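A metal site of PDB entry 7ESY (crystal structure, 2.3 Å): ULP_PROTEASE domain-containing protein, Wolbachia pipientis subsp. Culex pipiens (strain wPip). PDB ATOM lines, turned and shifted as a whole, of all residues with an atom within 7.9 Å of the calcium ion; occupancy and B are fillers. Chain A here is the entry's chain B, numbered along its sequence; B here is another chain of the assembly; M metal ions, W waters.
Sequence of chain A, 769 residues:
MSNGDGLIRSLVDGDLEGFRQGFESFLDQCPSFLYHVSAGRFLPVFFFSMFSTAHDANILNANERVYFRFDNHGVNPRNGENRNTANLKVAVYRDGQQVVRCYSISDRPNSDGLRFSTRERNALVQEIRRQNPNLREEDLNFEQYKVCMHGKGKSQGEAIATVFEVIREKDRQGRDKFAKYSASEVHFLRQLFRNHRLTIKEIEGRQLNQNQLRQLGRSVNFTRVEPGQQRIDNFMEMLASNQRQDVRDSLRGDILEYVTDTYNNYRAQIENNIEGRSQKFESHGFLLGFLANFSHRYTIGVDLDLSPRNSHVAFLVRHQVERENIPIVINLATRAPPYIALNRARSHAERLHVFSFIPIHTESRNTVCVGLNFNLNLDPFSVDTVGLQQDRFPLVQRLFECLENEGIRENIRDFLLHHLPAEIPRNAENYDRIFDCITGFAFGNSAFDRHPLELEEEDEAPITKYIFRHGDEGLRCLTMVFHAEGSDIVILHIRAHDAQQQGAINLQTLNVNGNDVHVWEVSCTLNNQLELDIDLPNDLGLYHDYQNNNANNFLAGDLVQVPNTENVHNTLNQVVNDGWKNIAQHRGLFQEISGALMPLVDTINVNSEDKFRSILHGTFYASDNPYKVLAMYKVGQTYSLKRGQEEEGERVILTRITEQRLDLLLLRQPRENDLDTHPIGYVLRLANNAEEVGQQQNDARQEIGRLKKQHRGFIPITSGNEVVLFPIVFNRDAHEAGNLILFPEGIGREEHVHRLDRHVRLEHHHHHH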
ATOM      1  N   GLN A 230     -29.603 -29.177  31.088  1.00  0.00           N
ATOM      2  CA  GLN A 230     -29.638 -28.632  29.733  1.00  0.00           C
ATOM      3  C   GLN A 230     -30.940 -29.032  29.046  1.00  0.00           C
ATOM      4  O   GLN A 230     -31.308 -30.211  29.019  1.00  0.00           O
ATOM      5  CB  GLN A 230     -28.441 -29.136  28.929  1.00  0.00           C
ATOM      6  CG  GLN A 230     -28.355 -28.633  27.503  1.00  0.00           C
ATOM      7  CD  GLN A 230     -27.146 -29.168  26.781  1.00  0.00           C
ATOM      8  OE1 GLN A 230     -26.588 -30.206  27.161  1.00  0.00           O
ATOM      9  NE2 GLN A 230     -26.714 -28.469  25.740  1.00  0.00           N
ATOM     10  N   ASP A 249     -22.826 -26.213  12.669  1.00  0.00           N
ATOM     11  CA  ASP A 249     -22.335 -25.675  13.938  1.00  0.00           C
ATOM     12  C   ASP A 249     -23.174 -26.155  15.120  1.00  0.00           C
ATOM     13  O   ASP A 249     -22.636 -26.365  16.212  1.00  0.00           O
ATOM     14  CB  ASP A 249     -22.304 -24.145  13.891  1.00  0.00           C
ATOM     15  CG  ASP A 249     -21.307 -23.631  12.872  1.00  0.00           C
ATOM     16  OD1 ASP A 249     -20.298 -24.336  12.612  1.00  0.00           O
ATOM     17  OD2 ASP A 249     -21.519 -22.528  12.330  1.00  0.00           O
ATOM     18  N   SER A 250     -24.491 -26.342  14.927  1.00  0.00           N
ATOM     19  CA  SER A 250     -25.316 -26.865  15.999  1.00  0.00           C
ATOM     20  C   SER A 250     -24.919 -28.287  16.357  1.00  0.00           C
ATOM     21  O   SER A 250     -24.929 -28.666  17.537  1.00  0.00           O
ATOM     22  CB  SER A 250     -26.791 -26.815  15.598  1.00  0.00           C
ATOM     23  OG  SER A 250     -27.060 -27.675  14.495  1.00  0.00           O
ATOM     24  N   LEU A 251     -24.562 -29.093  15.356  1.00  0.00           N
ATOM     25  CA  LEU A 251     -24.075 -30.448  15.630  1.00  0.00           C
ATOM     26  C   LEU A 251     -22.712 -30.427  16.321  1.00  0.00           C
ATOM     27  O   LEU A 251     -22.434 -31.291  17.165  1.00  0.00           O
ATOM     28  CB  LEU A 251     -24.006 -31.254  14.338  1.00  0.00           C
ATOM     29  CG  LEU A 251     -25.302 -31.777  13.718  1.00  0.00           C
ATOM     30  CD1 LEU A 251     -25.066 -32.143  12.252  1.00  0.00           C
ATOM     31  CD2 LEU A 251     -25.819 -32.978  14.482  1.00  0.00           C
ATOM     32  N   ARG A 252     -21.865 -29.454  15.977  1.00  0.00           N
ATOM     33  CA  ARG A 252     -20.503 -29.452  16.488  1.00  0.00           C
ATOM     34  C   ARG A 252     -20.450 -29.106  17.974  1.00  0.00           C
ATOM     35  O   ARG A 252     -19.766 -29.790  18.745  1.00  0.00           O
ATOM     36  CB  ARG A 252     -19.649 -28.465  15.690  1.00  0.00           C
ATOM     37  CG  ARG A 252     -18.970 -29.060  14.482  1.00  0.00           C
ATOM     38  CD  ARG A 252     -18.062 -28.040  13.837  1.00  0.00           C
ATOM     39  NE  ARG A 252     -17.433 -28.560  12.631  1.00  0.00           N
ATOM     40  CZ  ARG A 252     -16.780 -27.817  11.747  1.00  0.00           C
ATOM     41  NH1 ARG A 252     -16.667 -26.500  11.945  1.00  0.00           N
ATOM     42  NH2 ARG A 252     -16.239 -28.366  10.672  1.00  0.00           N
ATOM     43  N   GLY A 253     -21.142 -28.043  18.382  1.00  0.00           N
ATOM     44  CA  GLY A 253     -21.019 -27.533  19.731  1.00  0.00           C
ATOM     45  C   GLY A 253     -22.203 -27.714  20.641  1.00  0.00           C
ATOM     46  O   GLY A 253     -22.234 -27.115  21.719  1.00  0.00           O
ATOM     47  N   ASP A 254     -23.188 -28.531  20.266  1.00  0.00           N
ATOM     48  CA  ASP A 254     -24.373 -28.663  21.103  1.00  0.00           C
ATOM     49  C   ASP A 254     -24.957 -30.079  21.061  1.00  0.00           C
ATOM     50  O   ASP A 254     -24.947 -30.786  22.075  1.00  0.00           O
ATOM     51  CB  ASP A 254     -25.440 -27.660  20.657  1.00  0.00           C
ATOM     52  CG  ASP A 254     -25.886 -26.744  21.782  1.00  0.00           C
ATOM     53  OD1 ASP A 254     -25.396 -26.923  22.919  1.00  0.00           O
ATOM     54  OD2 ASP A 254     -26.721 -25.847  21.540  1.00  0.00           O
ATOM     55  N   ILE A 255     -25.457 -30.484  19.897  1.00  0.00           N
ATOM     56  CA  ILE A 255     -26.300 -31.681  19.819  1.00  0.00           C
ATOM     57  C   ILE A 255     -25.475 -32.941  20.053  1.00  0.00           C
ATOM     58  O   ILE A 255     -25.840 -33.796  20.863  1.00  0.00           O
ATOM     59  CB  ILE A 255     -27.042 -31.718  18.480  1.00  0.00           C
ATOM     60  CG1 ILE A 255     -27.943 -30.484  18.357  1.00  0.00           C
ATOM     61  CG2 ILE A 255     -27.845 -33.000  18.353  1.00  0.00           C
ATOM     62  CD1 ILE A 255     -28.798 -30.470  17.127  1.00  0.00           C
ATOM     63  N   GLU A 257     -22.565 -33.236  21.484  1.00  0.00           N
ATOM     64  CA  GLU A 257     -22.061 -33.258  22.852  1.00  0.00           C
ATOM     65  C   GLU A 257     -23.118 -33.790  23.818  1.00  0.00           C
ATOM     66  O   GLU A 257     -22.805 -34.576  24.714  1.00  0.00           O
ATOM     67  CB  GLU A 257     -21.602 -31.867  23.272  1.00  0.00           C
ATOM     68  CG  GLU A 257     -21.159 -31.765  24.730  1.00  0.00           C
ATOM     69  CD  GLU A 257     -20.665 -30.388  25.096  1.00  0.00           C
ATOM     70  OE1 GLU A 257     -20.333 -30.162  26.287  1.00  0.00           O
ATOM     71  OE2 GLU A 257     -20.610 -29.520  24.197  1.00  0.00           O
ATOM     72  N   TYR A 258     -24.372 -33.378  23.636  1.00  0.00           N
ATOM     73  CA  TYR A 258     -25.438 -33.872  24.501  1.00  0.00           C
ATOM     74  C   TYR A 258     -25.629 -35.371  24.341  1.00  0.00           C
ATOM     75  O   TYR A 258     -25.778 -36.094  25.343  1.00  0.00           O
ATOM     76  CB  TYR A 258     -26.749 -33.140  24.216  1.00  0.00           C
ATOM     77  CG  TYR A 258     -27.924 -33.764  24.918  1.00  0.00           C
ATOM     78  CD1 TYR A 258     -28.178 -33.494  26.259  1.00  0.00           C
ATOM     79  CD2 TYR A 258     -28.778 -34.640  24.261  1.00  0.00           C
ATOM     80  CE1 TYR A 258     -29.237 -34.072  26.926  1.00  0.00           C
ATOM     81  CE2 TYR A 258     -29.843 -35.227  24.918  1.00  0.00           C
ATOM     82  CZ  TYR A 258     -30.075 -34.936  26.246  1.00  0.00           C
ATOM     83  OH  TYR A 258     -31.134 -35.514  26.903  1.00  0.00           O
ATOM     84  N   ASP A 261     -22.694 -37.272  25.927  1.00  0.00           N
ATOM     85  CA  ASP A 261     -22.713 -37.131  27.382  1.00  0.00           C
ATOM     86  C   ASP A 261     -23.800 -37.997  28.007  1.00  0.00           C
ATOM     87  O   ASP A 261     -23.577 -38.636  29.036  1.00  0.00           O
ATOM     88  CB  ASP A 261     -22.898 -35.674  27.765  1.00  0.00           C
ATOM     89  CG  ASP A 261     -21.604 -34.883  27.706  1.00  0.00           C
ATOM     90  OD1 ASP A 261     -20.541 -35.499  27.487  1.00  0.00           O
ATOM     91  OD2 ASP A 261     -21.663 -33.646  27.877  1.00  0.00           O
ATOM     92  N   PHE A 381     -16.402 -37.378  18.220  1.00  0.00           N
ATOM     93  CA  PHE A 381     -17.067 -37.046  16.973  1.00  0.00           C
ATOM     94  C   PHE A 381     -16.300 -35.957  16.239  1.00  0.00           C
ATOM     95  O   PHE A 381     -15.522 -35.208  16.831  1.00  0.00           O
ATOM     96  CB  PHE A 381     -18.521 -36.614  17.194  1.00  0.00           C
ATOM     97  CG  PHE A 381     -18.685 -35.483  18.156  1.00  0.00           C
ATOM     98  CD1 PHE A 381     -18.618 -34.166  17.725  1.00  0.00           C
ATOM     99  CD2 PHE A 381     -18.928 -35.724  19.504  1.00  0.00           C
ATOM    100  CE1 PHE A 381     -18.776 -33.116  18.611  1.00  0.00           C
ATOM    101  CE2 PHE A 381     -19.082 -34.687  20.390  1.00  0.00           C
ATOM    102  CZ  PHE A 381     -19.008 -33.376  19.948  1.00  0.00           C
ATOM    103  N   TYR B 341     -26.163 -24.314  28.980  1.00  0.00           N
ATOM    104  CA  TYR B 341     -24.995 -25.185  28.864  1.00  0.00           C
ATOM    105  C   TYR B 341     -24.299 -25.036  27.503  1.00  0.00           C
ATOM    106  O   TYR B 341     -23.730 -25.998  26.982  1.00  0.00           O
ATOM    107  CB  TYR B 341     -25.381 -26.655  29.106  1.00  0.00           C
ATOM    108  CG  TYR B 341     -24.237 -27.557  29.508  1.00  0.00           C
ATOM    109  CD1 TYR B 341     -23.639 -27.437  30.757  1.00  0.00           C
ATOM    110  CD2 TYR B 341     -23.768 -28.548  28.646  1.00  0.00           C
ATOM    111  CE1 TYR B 341     -22.594 -28.264  31.125  1.00  0.00           C
ATOM    112  CE2 TYR B 341     -22.728 -29.383  29.015  1.00  0.00           C
ATOM    113  CZ  TYR B 341     -22.147 -29.232  30.255  1.00  0.00           C
ATOM    114  OH  TYR B 341     -21.111 -30.055  30.623  1.00  0.00           O
ATOM    115  N   THR B 342     -24.334 -23.840  26.928  1.00  0.00           N
ATOM    116  CA  THR B 342     -23.661 -23.622  25.657  1.00  0.00           C
ATOM    117  C   THR B 342     -23.375 -22.134  25.475  1.00  0.00           C
ATOM    118  O   THR B 342     -24.099 -21.282  25.989  1.00  0.00           O
ATOM    119  CB  THR B 342     -24.476 -24.154  24.473  1.00  0.00           C
ATOM    120  OG1 THR B 342     -23.707 -24.039  23.268  1.00  0.00           O
ATOM    121  CG2 THR B 342     -25.777 -23.380  24.306  1.00  0.00           C
ATOM    122  N   VAL B 343     -22.291 -21.852  24.761  1.00  0.00           N
ATOM    123  CA  VAL B 343     -21.930 -20.487  24.367  1.00  0.00           C
ATOM    124  C   VAL B 343     -21.980 -20.436  22.849  1.00  0.00           C
ATOM    125  O   VAL B 343     -21.436 -21.320  22.185  1.00  0.00           O
ATOM    126  CB  VAL B 343     -20.527 -20.085  24.862  1.00  0.00           C
ATOM    127  CG1 VAL B 343     -20.434 -18.577  25.031  1.00  0.00           C
ATOM    128  CG2 VAL B 343     -20.190 -20.803  26.164  1.00  0.00           C
ATOM    129  N   SER B 346     -18.487 -20.896  21.327  1.00  0.00           N
ATOM    130  CA  SER B 346     -17.565 -21.885  21.888  1.00  0.00           C
ATOM    131  C   SER B 346     -16.748 -22.556  20.791  1.00  0.00           C
ATOM    132  O   SER B 346     -15.563 -22.870  20.996  1.00  0.00           O
ATOM    133  CB  SER B 346     -18.320 -22.924  22.709  1.00  0.00           C
ATOM    134  OG  SER B 346     -19.118 -23.759  21.882  1.00  0.00           O
ATOM    135  N   GLY B 347     -17.356 -22.786  19.629  1.00  0.00           N
ATOM    136  CA  GLY B 347     -16.608 -23.352  18.514  1.00  0.00           C
ATOM    137  C   GLY B 347     -15.585 -22.385  17.960  1.00  0.00           C
ATOM    138  O   GLY B 347     -14.495 -22.784  17.555  1.00  0.00           O
ATOM    139  N   LYS B 395     -15.379 -24.001  31.098  1.00  0.00           N
ATOM    140  CA  LYS B 395     -15.578 -25.442  31.006  1.00  0.00           C
ATOM    141  C   LYS B 395     -16.172 -25.849  29.671  1.00  0.00           C
ATOM    142  O   LYS B 395     -15.865 -26.929  29.154  1.00  0.00           O
ATOM    143  CB  LYS B 395     -16.451 -25.918  32.162  1.00  0.00           C
ATOM    144  CG  LYS B 395     -15.892 -25.579  33.534  1.00  0.00           C
ATOM    145  CD  LYS B 395     -16.768 -26.116  34.643  1.00  0.00           C
ATOM    146  CE  LYS B 395     -16.899 -27.618  34.547  1.00  0.00           C
ATOM    147  NZ  LYS B 395     -15.563 -28.291  34.554  1.00  0.00           N
ATOM    148  N   LEU B 396     -17.027 -25.003  29.081  1.00  0.00           N
ATOM    149  CA  LEU B 396     -17.626 -25.344  27.803  1.00  0.00           C
ATOM    150  C   LEU B 396     -16.618 -25.263  26.665  1.00  0.00           C
ATOM    151  O   LEU B 396     -16.632 -26.084  25.745  1.00  0.00           O
ATOM    152  CB  LEU B 396     -18.824 -24.433  27.527  1.00  0.00           C
ATOM    153  CG  LEU B 396     -19.961 -24.561  28.530  1.00  0.00           C
ATOM    154  CD1 LEU B 396     -21.088 -23.602  28.214  1.00  0.00           C
ATOM    155  CD2 LEU B 396     -20.478 -25.993  28.573  1.00  0.00           C
ATOM    156  N   ILE B 397     -15.712 -24.278  26.717  1.00  0.00           N
ATOM    157  CA  ILE B 397     -14.655 -24.187  25.705  1.00  0.00           C
ATOM    158  C   ILE B 397     -13.723 -25.383  25.813  1.00  0.00           C
ATOM    159  O   ILE B 397     -13.265 -25.925  24.797  1.00  0.00           O
ATOM    160  CB  ILE B 397     -13.904 -22.854  25.835  1.00  0.00           C
ATOM    161  CG1 ILE B 397     -14.563 -21.768  24.979  1.00  0.00           C
ATOM    162  CG2 ILE B 397     -12.439 -23.000  25.446  1.00  0.00           C
ATOM    163  CD1 ILE B 397     -15.949 -21.348  25.434  1.00  0.00           C
ATOM    164  N   ARG B 399     -14.515 -28.430  26.999  1.00  0.00           N
ATOM    165  CA  ARG B 399     -15.241 -29.590  26.494  1.00  0.00           C
ATOM    166  C   ARG B 399     -15.334 -29.572  24.972  1.00  0.00           C
ATOM    167  O   ARG B 399     -15.291 -30.635  24.331  1.00  0.00           O
ATOM    168  CB  ARG B 399     -16.631 -29.666  27.118  1.00  0.00           C
ATOM    169  CG  ARG B 399     -16.625 -29.936  28.623  1.00  0.00           C
ATOM    170  CD  ARG B 399     -16.048 -31.302  28.939  1.00  0.00           C
ATOM    171  NE  ARG B 399     -16.916 -32.389  28.475  1.00  0.00           N
ATOM    172  CZ  ARG B 399     -16.546 -33.661  28.405  1.00  0.00           C
ATOM    173  NH1 ARG B 399     -15.318 -34.018  28.748  1.00  0.00           N
ATOM    174  NH2 ARG B 399     -17.397 -34.582  27.971  1.00  0.00           N
ATOM    175  N   ASP B 400     -15.471 -28.391  24.379  1.00  0.00           N
ATOM    176  CA  ASP B 400     -15.490 -28.293  22.915  1.00  0.00           C
ATOM    177  C   ASP B 400     -14.165 -28.741  22.316  1.00  0.00           C
ATOM    178  O   ASP B 400     -14.134 -29.448  21.304  1.00  0.00           O
ATOM    179  CB  ASP B 400     -15.817 -26.860  22.489  1.00  0.00           C
ATOM    180  CG  ASP B 400     -17.292 -26.644  22.230  1.00  0.00           C
ATOM    181  OD1 ASP B 400     -18.107 -27.060  23.084  1.00  0.00           O
ATOM    182  OD2 ASP B 400     -17.635 -26.054  21.186  1.00  0.00           O
ATOM    183  N   LEU B 401     -13.051 -28.337  22.932  1.00  0.00           N
ATOM    184  CA  LEU B 401     -11.736 -28.734  22.432  1.00  0.00           C
ATOM    185  C   LEU B 401     -11.447 -30.212  22.674  1.00  0.00           C
ATOM    186  O   LEU B 401     -10.521 -30.752  22.052  1.00  0.00           O
ATOM    187  CB  LEU B 401     -10.649 -27.874  23.076  1.00  0.00           C
ATOM    188  CG  LEU B 401     -10.467 -26.461  22.537  1.00  0.00           C
ATOM    189  CD1 LEU B 401      -9.564 -25.653  23.445  1.00  0.00           C
ATOM    190  CD2 LEU B 401      -9.907 -26.506  21.131  1.00  0.00           C
ATOM    191  N   LEU B 403     -14.054 -32.751  22.685  1.00  0.00           N
ATOM    192  CA  LEU B 403     -15.080 -33.643  22.157  1.00  0.00           C
ATOM    193  C   LEU B 403     -15.238 -33.578  20.639  1.00  0.00           C
ATOM    194  O   LEU B 403     -15.816 -34.505  20.066  1.00  0.00           O
ATOM    195  CB  LEU B 403     -16.435 -33.334  22.797  1.00  0.00           C
ATOM    196  CG  LEU B 403     -16.594 -33.688  24.273  1.00  0.00           C
ATOM    197  CD1 LEU B 403     -18.027 -33.495  24.725  1.00  0.00           C
ATOM    198  CD2 LEU B 403     -16.138 -35.118  24.544  1.00  0.00           C
HETATM  199 CA    CA M   1     -20.500 -27.198  23.515  1.00  0.00          CA
HETATM  200  O   HOH W   1     -21.150 -24.646  23.565  1.00  0.00           O
HETATM  201  O   HOH W   2     -18.904 -27.484  25.477  1.00  0.00           O
HETATM  202  O   HOH W   3     -22.747 -27.702  24.676  1.00  0.00           O
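Water W2 bridges O of Leu 396 of chain B (2.7 Å) and OE1 of Glu 257 (3.1 Å).
Water W1 lies within hydrogen-bond range of OG1 of Thr 342 of chain B (2.6 Å), OG of Ser 346 of chain B (2.8 Å) and N of Val 343 of chain B (3.2 Å).
Water W3 lies within hydrogen-bond range of O of Tyr 341 of chain B and OD1 of Asp 254.
OG of Ser 346 of chain B lies within hydrogen-bond range of OD2 of Asp 400 of chain B.
The calcium ion is bound by OE2 of Glu 257 (2.4 Å).
OD1 of Asp 400 of chain B is bound to the calcium ion (2.4 Å).
O of Gly 253 is bound to the calcium ion (2.5 Å).
Water W2 is bound to the calcium ion (2.5 Å).
The calcium ion is bound by water W3, 2.6 Å away.
The calcium ion is bound by water W1, at 2.6 Å.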
